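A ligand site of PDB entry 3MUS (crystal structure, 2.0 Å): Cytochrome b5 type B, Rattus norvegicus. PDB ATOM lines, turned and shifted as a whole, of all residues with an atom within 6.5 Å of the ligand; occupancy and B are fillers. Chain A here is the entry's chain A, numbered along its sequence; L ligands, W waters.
FE1 of the ligand is bound by NE2 of His 39 (2.1 Å).
NE2 of His 63 binds FE1 of the ligand, 2.1 Å away.
An oxygen (O2) of the ligand lies within hydrogen-bond range of the backbone NH (N) of Ser 64, at 2.9 Å.
The side-chain hydroxyl (OG) of Ser 64 is in hydrogen-bond range of an oxygen (O1) of the ligand (2.7 Å).
ND1 of His 39 is in hydrogen-bond range of O of Gly 42.
A ring nitrogen (ND1) of His 63 lies within hydrogen-bond range of the backbone carbonyl oxygen (O) of Phe 58, at 2.7 Å.
The backbone NH of Ala 67 sits at hydrogen-bond distance from the side-chain hydroxyl of Ser 64, at 3.0 Å.
The side-chain hydroxyl (OG) of Ser 64 lies close to the backbone NH (N) of Asp 66, 3.1 Å away.
OG of Ser 57 sits at hydrogen-bond distance from OE1 of Gln 49 (3.0 Å).
N of Tyr 30 sits at hydrogen-bond distance from O of Met 23, at 2.8 Å.
Merely in contact with the ligand: Met 23 (3.9 Å), Ile 25 (3.9 Å), Ile 32 (3.5 Å), Phe 35 (3.5 Å), Pro 40 (3.6 Å), Gly 41 (3.7 Å), Val 45 (3.95 Å), Leu 46 (3.6 Å), Ser 57 (3.4 Å), Phe 58 (3.7 Å), Val 61 (3.6 Å), Ala 67 (3.7 Å), Met 70 (3.7 Å) and Leu 71 (3.7 Å).
Hydrophobic or aromatic side chains within 4 Å of the ligand: Met 23, Ile 25, Ile 32, Phe 35, His 39, Pro 40, Val 45, Leu 46, Phe 58, Val 61, His 63, Ala 67, Met 70 and Leu 71.
Within 4 Å of the ligand: Met 23, Ile 25, Ile 32, Phe 35, His 39, Pro 40, Gly 41, Val 45, Leu 46, Ser 57, Phe 58, Val 61, His 63, Ser 64, Ala 67, Met 70 and Leu 71.
The nearest printed residue that does not touch the ligand is Ala 54 (4.05 Å).
Water W1 bridges O of Gly 62 (2.8 Å) and O2 of the ligand (3.2 Å).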
ATOM      1  N   MET A  23      12.307  18.548 -13.238  1.00  0.00           N
ATOM      2  CA  MET A  23      11.625  18.354 -11.998  1.00  0.00           C
ATOM      3  C   MET A  23      12.104  17.015 -11.421  1.00  0.00           C
ATOM      4  O   MET A  23      12.422  16.083 -12.173  1.00  0.00           O
ATOM      5  CB  MET A  23      10.124  18.347 -12.298  1.00  0.00           C
ATOM      6  CG  MET A  23       9.194  17.968 -11.203  1.00  0.00           C
ATOM      7  SD  MET A  23       7.457  18.153 -11.843  1.00  0.00           S
ATOM      8  CE  MET A  23       7.255  19.870 -11.790  1.00  0.00           C
ATOM      9  N   ILE A  25      11.036  13.778  -9.057  1.00  0.00           N
ATOM     10  CA  ILE A  25       9.952  12.992  -8.513  1.00  0.00           C
ATOM     11  C   ILE A  25      10.544  11.633  -8.008  1.00  0.00           C
ATOM     12  O   ILE A  25      11.169  10.913  -8.781  1.00  0.00           O
ATOM     13  CB  ILE A  25       8.854  12.734  -9.587  1.00  0.00           C
ATOM     14  CG1 ILE A  25       8.232  14.077 -10.016  1.00  0.00           C
ATOM     15  CG2 ILE A  25       7.754  11.840  -8.982  1.00  0.00           C
ATOM     16  CD1 ILE A  25       7.128  13.905 -11.104  1.00  0.00           C
ATOM     17  N   TYR A  30      13.335  14.404 -14.272  1.00  0.00           N
ATOM     18  CA  TYR A  30      12.559  14.355 -15.495  1.00  0.00           C
ATOM     19  C   TYR A  30      12.606  15.696 -16.232  1.00  0.00           C
ATOM     20  O   TYR A  30      12.371  16.755 -15.644  1.00  0.00           O
ATOM     21  CB  TYR A  30      11.082  14.030 -15.202  1.00  0.00           C
ATOM     22  CG  TYR A  30      10.904  12.730 -14.525  1.00  0.00           C
ATOM     23  CD1 TYR A  30      11.003  12.638 -13.131  1.00  0.00           C
ATOM     24  CD2 TYR A  30      10.732  11.571 -15.269  1.00  0.00           C
ATOM     25  CE1 TYR A  30      10.936  11.390 -12.513  1.00  0.00           C
ATOM     26  CE2 TYR A  30      10.662  10.314 -14.678  1.00  0.00           C
ATOM     27  CZ  TYR A  30      10.760  10.226 -13.293  1.00  0.00           C
ATOM     28  OH  TYR A  30      10.694   8.974 -12.666  1.00  0.00           O
ATOM     29  N   ILE A  32      10.614  17.815 -18.351  1.00  0.00           N
ATOM     30  CA  ILE A  32       9.219  17.887 -18.808  1.00  0.00           C
ATOM     31  C   ILE A  32       8.949  19.110 -19.713  1.00  0.00           C
ATOM     32  O   ILE A  32       7.799  19.483 -19.923  1.00  0.00           O
ATOM     33  CB  ILE A  32       8.210  17.901 -17.583  1.00  0.00           C
ATOM     34  CG1 ILE A  32       8.512  19.050 -16.616  1.00  0.00           C
ATOM     35  CG2 ILE A  32       8.263  16.567 -16.858  1.00  0.00           C
ATOM     36  CD1 ILE A  32       7.303  19.465 -15.814  1.00  0.00           C
ATOM     37  N   PHE A  35       6.310  18.588 -22.271  1.00  0.00           N
ATOM     38  CA  PHE A  35       5.032  18.166 -21.718  1.00  0.00           C
ATOM     39  C   PHE A  35       4.153  19.324 -21.149  1.00  0.00           C
ATOM     40  O   PHE A  35       2.938  19.167 -20.925  1.00  0.00           O
ATOM     41  CB  PHE A  35       5.343  17.160 -20.621  1.00  0.00           C
ATOM     42  CG  PHE A  35       4.126  16.540 -20.007  1.00  0.00           C
ATOM     43  CD1 PHE A  35       3.226  15.802 -20.789  1.00  0.00           C
ATOM     44  CD2 PHE A  35       3.907  16.648 -18.633  1.00  0.00           C
ATOM     45  CE1 PHE A  35       2.119  15.157 -20.193  1.00  0.00           C
ATOM     46  CE2 PHE A  35       2.818  16.018 -18.044  1.00  0.00           C
ATOM     47  CZ  PHE A  35       1.920  15.266 -18.821  1.00  0.00           C
ATOM     48  N   HIS A  39       0.092  18.747 -20.398  1.00  0.00           N
ATOM     49  CA  HIS A  39      -0.341  18.299 -19.075  1.00  0.00           C
ATOM     50  C   HIS A  39      -1.842  18.545 -18.763  1.00  0.00           C
ATOM     51  O   HIS A  39      -2.294  19.678 -18.748  1.00  0.00           O
ATOM     52  CB  HIS A  39       0.513  19.007 -18.031  1.00  0.00           C
ATOM     53  CG  HIS A  39       0.167  18.609 -16.630  1.00  0.00           C
ATOM     54  ND1 HIS A  39      -0.007  19.536 -15.621  1.00  0.00           N
ATOM     55  CD2 HIS A  39      -0.010  17.391 -16.071  1.00  0.00           C
ATOM     56  CE1 HIS A  39      -0.291  18.896 -14.496  1.00  0.00           C
ATOM     57  NE2 HIS A  39      -0.302  17.592 -14.751  1.00  0.00           N
ATOM     58  N   PRO A  40      -2.616  17.497 -18.455  1.00  0.00           N
ATOM     59  CA  PRO A  40      -4.037  17.793 -18.198  1.00  0.00           C
ATOM     60  C   PRO A  40      -4.341  18.774 -17.074  1.00  0.00           C
ATOM     61  O   PRO A  40      -5.368  19.437 -17.125  1.00  0.00           O
ATOM     62  CB  PRO A  40      -4.657  16.401 -17.962  1.00  0.00           C
ATOM     63  CG  PRO A  40      -3.799  15.525 -18.804  1.00  0.00           C
ATOM     64  CD  PRO A  40      -2.378  16.051 -18.560  1.00  0.00           C
ATOM     65  N   GLY A  41      -3.480  18.842 -16.046  1.00  0.00           N
ATOM     66  CA  GLY A  41      -3.681  19.812 -14.989  1.00  0.00           C
ATOM     67  C   GLY A  41      -3.193  21.241 -15.299  1.00  0.00           C
ATOM     68  O   GLY A  41      -3.278  22.107 -14.413  1.00  0.00           O
ATOM     69  N   GLY A  42      -2.683  21.488 -16.508  1.00  0.00           N
ATOM     70  CA  GLY A  42      -2.250  22.824 -16.901  1.00  0.00           C
ATOM     71  C   GLY A  42      -0.751  23.042 -16.756  1.00  0.00           C
ATOM     72  O   GLY A  42      -0.044  22.255 -16.097  1.00  0.00           O
ATOM     73  N   VAL A  45       0.817  24.801 -12.691  1.00  0.00           N
ATOM     74  CA  VAL A  45       1.175  23.995 -11.524  1.00  0.00           C
ATOM     75  C   VAL A  45       2.535  23.341 -11.713  1.00  0.00           C
ATOM     76  O   VAL A  45       3.225  23.125 -10.743  1.00  0.00           O
ATOM     77  CB  VAL A  45       0.083  22.927 -11.176  1.00  0.00           C
ATOM     78  CG1 VAL A  45      -1.222  23.652 -10.836  1.00  0.00           C
ATOM     79  CG2 VAL A  45      -0.158  21.953 -12.381  1.00  0.00           C
ATOM     80  N   LEU A  46       2.944  23.061 -12.943  1.00  0.00           N
ATOM     81  CA  LEU A  46       4.292  22.500 -13.185  1.00  0.00           C
ATOM     82  C   LEU A  46       5.390  23.590 -13.061  1.00  0.00           C
ATOM     83  O   LEU A  46       6.453  23.371 -12.422  1.00  0.00           O
ATOM     84  CB  LEU A  46       4.369  21.824 -14.607  1.00  0.00           C
ATOM     85  CG  LEU A  46       3.320  20.744 -14.972  1.00  0.00           C
ATOM     86  CD1 LEU A  46       3.457  20.255 -16.389  1.00  0.00           C
ATOM     87  CD2 LEU A  46       3.416  19.599 -14.046  1.00  0.00           C
ATOM     88  N   GLN A  49       6.608  24.532  -9.710  1.00  0.00           N
ATOM     89  CA  GLN A  49       7.453  23.552  -9.090  1.00  0.00           C
ATOM     90  C   GLN A  49       8.680  23.201  -9.954  1.00  0.00           C
ATOM     91  O   GLN A  49       9.388  22.254  -9.691  1.00  0.00           O
ATOM     92  CB  GLN A  49       6.589  22.328  -8.856  1.00  0.00           C
ATOM     93  CG  GLN A  49       6.880  21.643  -7.596  1.00  0.00           C
ATOM     94  CD  GLN A  49       5.801  21.855  -6.588  1.00  0.00           C
ATOM     95  OE1 GLN A  49       5.812  21.234  -5.523  1.00  0.00           O
ATOM     96  NE2 GLN A  49       4.849  22.729  -6.906  1.00  0.00           N
ATOM     97  N   ALA A  54       9.211  17.667  -6.683  1.00  0.00           N
ATOM     98  CA  ALA A  54       7.769  17.810  -6.680  1.00  0.00           C
ATOM     99  C   ALA A  54       7.017  16.534  -6.229  1.00  0.00           C
ATOM    100  O   ALA A  54       5.812  16.415  -6.394  1.00  0.00           O
ATOM    101  CB  ALA A  54       7.290  18.274  -8.101  1.00  0.00           C
ATOM    102  N   SER A  57       3.632  17.021  -4.138  1.00  0.00           N
ATOM    103  CA  SER A  57       2.484  17.530  -4.912  1.00  0.00           C
ATOM    104  C   SER A  57       1.981  16.485  -5.909  1.00  0.00           C
ATOM    105  O   SER A  57       0.773  16.263  -6.068  1.00  0.00           O
ATOM    106  CB  SER A  57       2.870  18.789  -5.642  1.00  0.00           C
ATOM    107  OG  SER A  57       3.280  19.743  -4.710  1.00  0.00           O
ATOM    108  N   PHE A  58       2.915  15.842  -6.590  1.00  0.00           N
ATOM    109  CA  PHE A  58       2.551  14.792  -7.531  1.00  0.00           C
ATOM    110  C   PHE A  58       1.682  13.736  -6.851  1.00  0.00           C
ATOM    111  O   PHE A  58       0.640  13.288  -7.409  1.00  0.00           O
ATOM    112  CB  PHE A  58       3.818  14.102  -8.074  1.00  0.00           C
ATOM    113  CG  PHE A  58       3.521  13.016  -9.055  1.00  0.00           C
ATOM    114  CD1 PHE A  58       3.266  13.322 -10.386  1.00  0.00           C
ATOM    115  CD2 PHE A  58       3.474  11.681  -8.643  1.00  0.00           C
ATOM    116  CE1 PHE A  58       2.960  12.348 -11.299  1.00  0.00           C
ATOM    117  CE2 PHE A  58       3.160  10.656  -9.568  1.00  0.00           C
ATOM    118  CZ  PHE A  58       2.903  10.976 -10.903  1.00  0.00           C
ATOM    119  N   VAL A  61      -1.950  14.918  -5.503  1.00  0.00           N
ATOM    120  CA  VAL A  61      -3.003  15.062  -6.508  1.00  0.00           C
ATOM    121  C   VAL A  61      -3.709  13.720  -6.684  1.00  0.00           C
ATOM    122  O   VAL A  61      -4.909  13.651  -6.949  1.00  0.00           O
ATOM    123  CB  VAL A  61      -2.402  15.512  -7.855  1.00  0.00           C
ATOM    124  CG1 VAL A  61      -3.448  15.424  -9.000  1.00  0.00           C
ATOM    125  CG2 VAL A  61      -1.856  16.925  -7.709  1.00  0.00           C
ATOM    126  N   GLY A  62      -2.984  12.631  -6.518  1.00  0.00           N
ATOM    127  CA  GLY A  62      -3.628  11.346  -6.743  1.00  0.00           C
ATOM    128  C   GLY A  62      -3.631  10.997  -8.237  1.00  0.00           C
ATOM    129  O   GLY A  62      -4.675  10.714  -8.813  1.00  0.00           O
ATOM    130  N   HIS A  63      -2.449  11.027  -8.858  1.00  0.00           N
ATOM    131  CA  HIS A  63      -2.299  10.687 -10.258  1.00  0.00           C
ATOM    132  C   HIS A  63      -2.617   9.212 -10.550  1.00  0.00           C
ATOM    133  O   HIS A  63      -2.318   8.332  -9.727  1.00  0.00           O
ATOM    134  CB  HIS A  63      -0.876  11.037 -10.734  1.00  0.00           C
ATOM    135  CG  HIS A  63      -0.663  12.503 -10.961  1.00  0.00           C
ATOM    136  ND1 HIS A  63      -0.240  13.363  -9.976  1.00  0.00           N
ATOM    137  CD2 HIS A  63      -0.839  13.271 -12.074  1.00  0.00           C
ATOM    138  CE1 HIS A  63      -0.135  14.590 -10.464  1.00  0.00           C
ATOM    139  NE2 HIS A  63      -0.503  14.554 -11.734  1.00  0.00           N
ATOM    140  N   SER A  64      -3.201   8.965 -11.711  1.00  0.00           N
ATOM    141  CA  SER A  64      -3.595   7.633 -12.134  1.00  0.00           C
ATOM    142  C   SER A  64      -2.388   6.769 -12.529  1.00  0.00           C
ATOM    143  O   SER A  64      -1.270   7.282 -12.774  1.00  0.00           O
ATOM    144  CB  SER A  64      -4.472   7.718 -13.377  1.00  0.00           C
ATOM    145  OG  SER A  64      -3.661   8.009 -14.498  1.00  0.00           O
ATOM    146  N   PRO A  65      -2.606   5.452 -12.667  1.00  0.00           N
ATOM    147  CA  PRO A  65      -1.514   4.589 -13.088  1.00  0.00           C
ATOM    148  C   PRO A  65      -1.048   5.017 -14.481  1.00  0.00           C
ATOM    149  O   PRO A  65       0.121   4.862 -14.820  1.00  0.00           O
ATOM    150  CB  PRO A  65      -2.149   3.192 -13.133  1.00  0.00           C
ATOM    151  CG  PRO A  65      -3.182   3.254 -12.072  1.00  0.00           C
ATOM    152  CD  PRO A  65      -3.796   4.646 -12.331  1.00  0.00           C
ATOM    153  N   ASP A  66      -1.960   5.528 -15.303  1.00  0.00           N
ATOM    154  CA  ASP A  66      -1.493   5.902 -16.634  1.00  0.00           C
ATOM    155  C   ASP A  66      -0.602   7.139 -16.561  1.00  0.00           C
ATOM    156  O   ASP A  66       0.284   7.287 -17.393  1.00  0.00           O
ATOM    157  CB  ASP A  66      -2.648   6.156 -17.591  1.00  0.00           C
ATOM    158  CG  ASP A  66      -3.389   4.874 -17.935  1.00  0.00           C
ATOM    159  OD1 ASP A  66      -2.772   3.920 -18.485  1.00  0.00           O
ATOM    160  OD2 ASP A  66      -4.599   4.821 -17.626  1.00  0.00           O
ATOM    161  N   ALA A  67      -0.850   8.021 -15.596  1.00  0.00           N
ATOM    162  CA  ALA A  67       0.002   9.221 -15.446  1.00  0.00           C
ATOM    163  C   ALA A  67       1.445   8.789 -15.029  1.00  0.00           C
ATOM    164  O   ALA A  67       2.438   9.368 -15.516  1.00  0.00           O
ATOM    165  CB  ALA A  67      -0.633  10.191 -14.389  1.00  0.00           C
ATOM    166  N   ARG A  68       1.547   7.780 -14.150  1.00  0.00           N
ATOM    167  CA  ARG A  68       2.874   7.256 -13.727  1.00  0.00           C
ATOM    168  C   ARG A  68       3.618   6.701 -14.921  1.00  0.00           C
ATOM    169  O   ARG A  68       4.822   6.956 -15.095  1.00  0.00           O
ATOM    170  CB  ARG A  68       2.752   6.147 -12.670  1.00  0.00           C
ATOM    171  CG  ARG A  68       2.272   6.650 -11.328  1.00  0.00           C
ATOM    172  CD  ARG A  68       2.204   5.572 -10.310  1.00  0.00           C
ATOM    173  NE  ARG A  68       1.463   6.046  -9.134  1.00  0.00           N
ATOM    174  CZ  ARG A  68       1.983   6.779  -8.161  1.00  0.00           C
ATOM    175  NH1 ARG A  68       3.272   7.132  -8.174  1.00  0.00           N
ATOM    176  NH2 ARG A  68       1.207   7.166  -7.146  1.00  0.00           N
ATOM    177  N   MET A  70       3.413   7.577 -18.063  1.00  0.00           N
ATOM    178  CA  MET A  70       3.909   8.686 -18.873  1.00  0.00           C
ATOM    179  C   MET A  70       5.296   9.192 -18.431  1.00  0.00           C
ATOM    180  O   MET A  70       6.059   9.717 -19.258  1.00  0.00           O
ATOM    181  CB  MET A  70       2.925   9.853 -18.814  1.00  0.00           C
ATOM    182  CG  MET A  70       1.634   9.573 -19.509  1.00  0.00           C
ATOM    183  SD  MET A  70       0.619  11.047 -19.461  1.00  0.00           S
ATOM    184  CE  MET A  70       1.434  12.007 -20.621  1.00  0.00           C
ATOM    185  N   LEU A  71       5.615   9.077 -17.149  1.00  0.00           N
ATOM    186  CA  LEU A  71       6.916   9.555 -16.674  1.00  0.00           C
ATOM    187  C   LEU A  71       8.081   9.030 -17.479  1.00  0.00           C
ATOM    188  O   LEU A  71       9.010   9.783 -17.823  1.00  0.00           O
ATOM    189  CB  LEU A  71       7.111   9.186 -15.218  1.00  0.00           C
ATOM    190  CG  LEU A  71       6.344  10.099 -14.270  1.00  0.00           C
ATOM    191  CD1 LEU A  71       6.519   9.585 -12.884  1.00  0.00           C
ATOM    192  CD2 LEU A  71       6.918  11.510 -14.388  1.00  0.00           C
ATOM    193  N   TYR A  74      10.106  10.893 -19.979  1.00  0.00           N
ATOM    194  CA  TYR A  74      10.815  12.142 -19.658  1.00  0.00           C
ATOM    195  C   TYR A  74      11.996  11.912 -18.727  1.00  0.00           C
ATOM    196  O   TYR A  74      12.702  12.841 -18.350  1.00  0.00           O
ATOM    197  CB  TYR A  74       9.832  13.145 -19.026  1.00  0.00           C
ATOM    198  CG  TYR A  74       8.617  13.382 -19.904  1.00  0.00           C
ATOM    199  CD1 TYR A  74       8.764  14.000 -21.164  1.00  0.00           C
ATOM    200  CD2 TYR A  74       7.358  12.948 -19.529  1.00  0.00           C
ATOM    201  CE1 TYR A  74       7.697  14.165 -22.032  1.00  0.00           C
ATOM    202  CE2 TYR A  74       6.228  13.110 -20.412  1.00  0.00           C
ATOM    203  CZ  TYR A  74       6.439  13.719 -21.653  1.00  0.00           C
ATOM    204  OH  TYR A  74       5.384  13.893 -22.496  1.00  0.00           O
HETATM  205  C1  LIG L   1      -3.765  15.659 -14.014  1.00  0.00           C
HETATM  206  C2  LIG L   1       0.319  13.691 -15.690  1.00  0.00           C
HETATM  207  C3  LIG L   1       2.896  16.327 -12.575  1.00  0.00           C
HETATM  208  C4  LIG L   1      -1.141  18.401 -10.954  1.00  0.00           C
HETATM  209  C5  LIG L   1      -2.867  14.861 -14.744  1.00  0.00           C
HETATM  210  C6  LIG L   1      -3.239  13.837 -15.649  1.00  0.00           C
HETATM  211  C7  LIG L   1      -2.089  13.319 -16.155  1.00  0.00           C
HETATM  212  C8  LIG L   1      -1.009  13.989 -15.503  1.00  0.00           C
HETATM  213  C9  LIG L   1      -1.994  12.266 -17.135  1.00  0.00           C
HETATM  214  C10 LIG L   1      -4.674  13.373 -15.973  1.00  0.00           C
HETATM  215  C11 LIG L   1      -5.360  12.596 -14.820  1.00  0.00           C
HETATM  216  C12 LIG L   1      -4.593  11.325 -14.401  1.00  0.00           C
HETATM  217  O1  LIG L   1      -4.296  10.477 -15.277  1.00  0.00           O
HETATM  218  O2  LIG L   1      -4.311  11.168 -13.192  1.00  0.00           O
HETATM  219  C13 LIG L   1       1.340  14.267 -14.986  1.00  0.00           C
HETATM  220  C14 LIG L   1       2.716  13.941 -15.205  1.00  0.00           C
HETATM  221  C15 LIG L   1       3.474  14.657 -14.356  1.00  0.00           C
HETATM  222  C16 LIG L   1       2.520  15.451 -13.597  1.00  0.00           C
HETATM  223  C17 LIG L   1       3.227  12.932 -16.229  1.00  0.00           C
HETATM  224  C18 LIG L   1       4.926  14.581 -14.248  1.00  0.00           C
HETATM  225  C19 LIG L   1       5.628  15.823 -14.720  1.00  0.00           C
HETATM  226  C20 LIG L   1       2.049  17.096 -11.855  1.00  0.00           C
HETATM  227  C21 LIG L   1       2.456  18.005 -10.810  1.00  0.00           C
HETATM  228  C22 LIG L   1       1.346  18.616 -10.332  1.00  0.00           C
HETATM  229  C23 LIG L   1       0.214  18.055 -11.112  1.00  0.00           C
HETATM  230  C24 LIG L   1       3.896  18.268 -10.305  1.00  0.00           C
HETATM  231  C25 LIG L   1       1.308  19.663  -9.228  1.00  0.00           C
HETATM  232  C26 LIG L   1       0.616  19.607  -8.087  1.00  0.00           C
HETATM  233  C27 LIG L   1      -2.226  17.834 -11.678  1.00  0.00           C
HETATM  234  C28 LIG L   1      -3.618  18.204 -11.479  1.00  0.00           C
HETATM  235  C29 LIG L   1      -4.359  17.431 -12.303  1.00  0.00           C
HETATM  236  C30 LIG L   1      -3.409  16.583 -13.044  1.00  0.00           C
HETATM  237  C31 LIG L   1      -4.147  19.257 -10.498  1.00  0.00           C
HETATM  238  C32 LIG L   1      -5.910  17.447 -12.425  1.00  0.00           C
HETATM  239  C33 LIG L   1      -6.491  16.248 -11.613  1.00  0.00           C
HETATM  240  C34 LIG L   1      -7.734  15.684 -12.231  1.00  0.00           C
HETATM  241  O3  LIG L   1      -7.641  14.721 -13.099  1.00  0.00           O
HETATM  242  O4  LIG L   1      -8.739  16.383 -12.086  1.00  0.00           O
HETATM  243  N1  LIG L   1      -1.490  14.933 -14.596  1.00  0.00           N
HETATM  244  N2  LIG L   1       1.213  15.215 -13.996  1.00  0.00           N
HETATM  245  N3  LIG L   1       0.661  17.123 -12.043  1.00  0.00           N
HETATM  246  N4  LIG L   1      -2.093  16.833 -12.650  1.00  0.00           N
HETATM  247 FE1  LIG L   1      -0.447  16.028 -13.297  1.00  0.00          FE
HETATM  248  O   HOH W   1      -6.081  12.193 -10.767  1.00  0.00           O
HETATM  249  O   HOH W   2      -5.328  10.530 -18.024  1.00  0.00           O
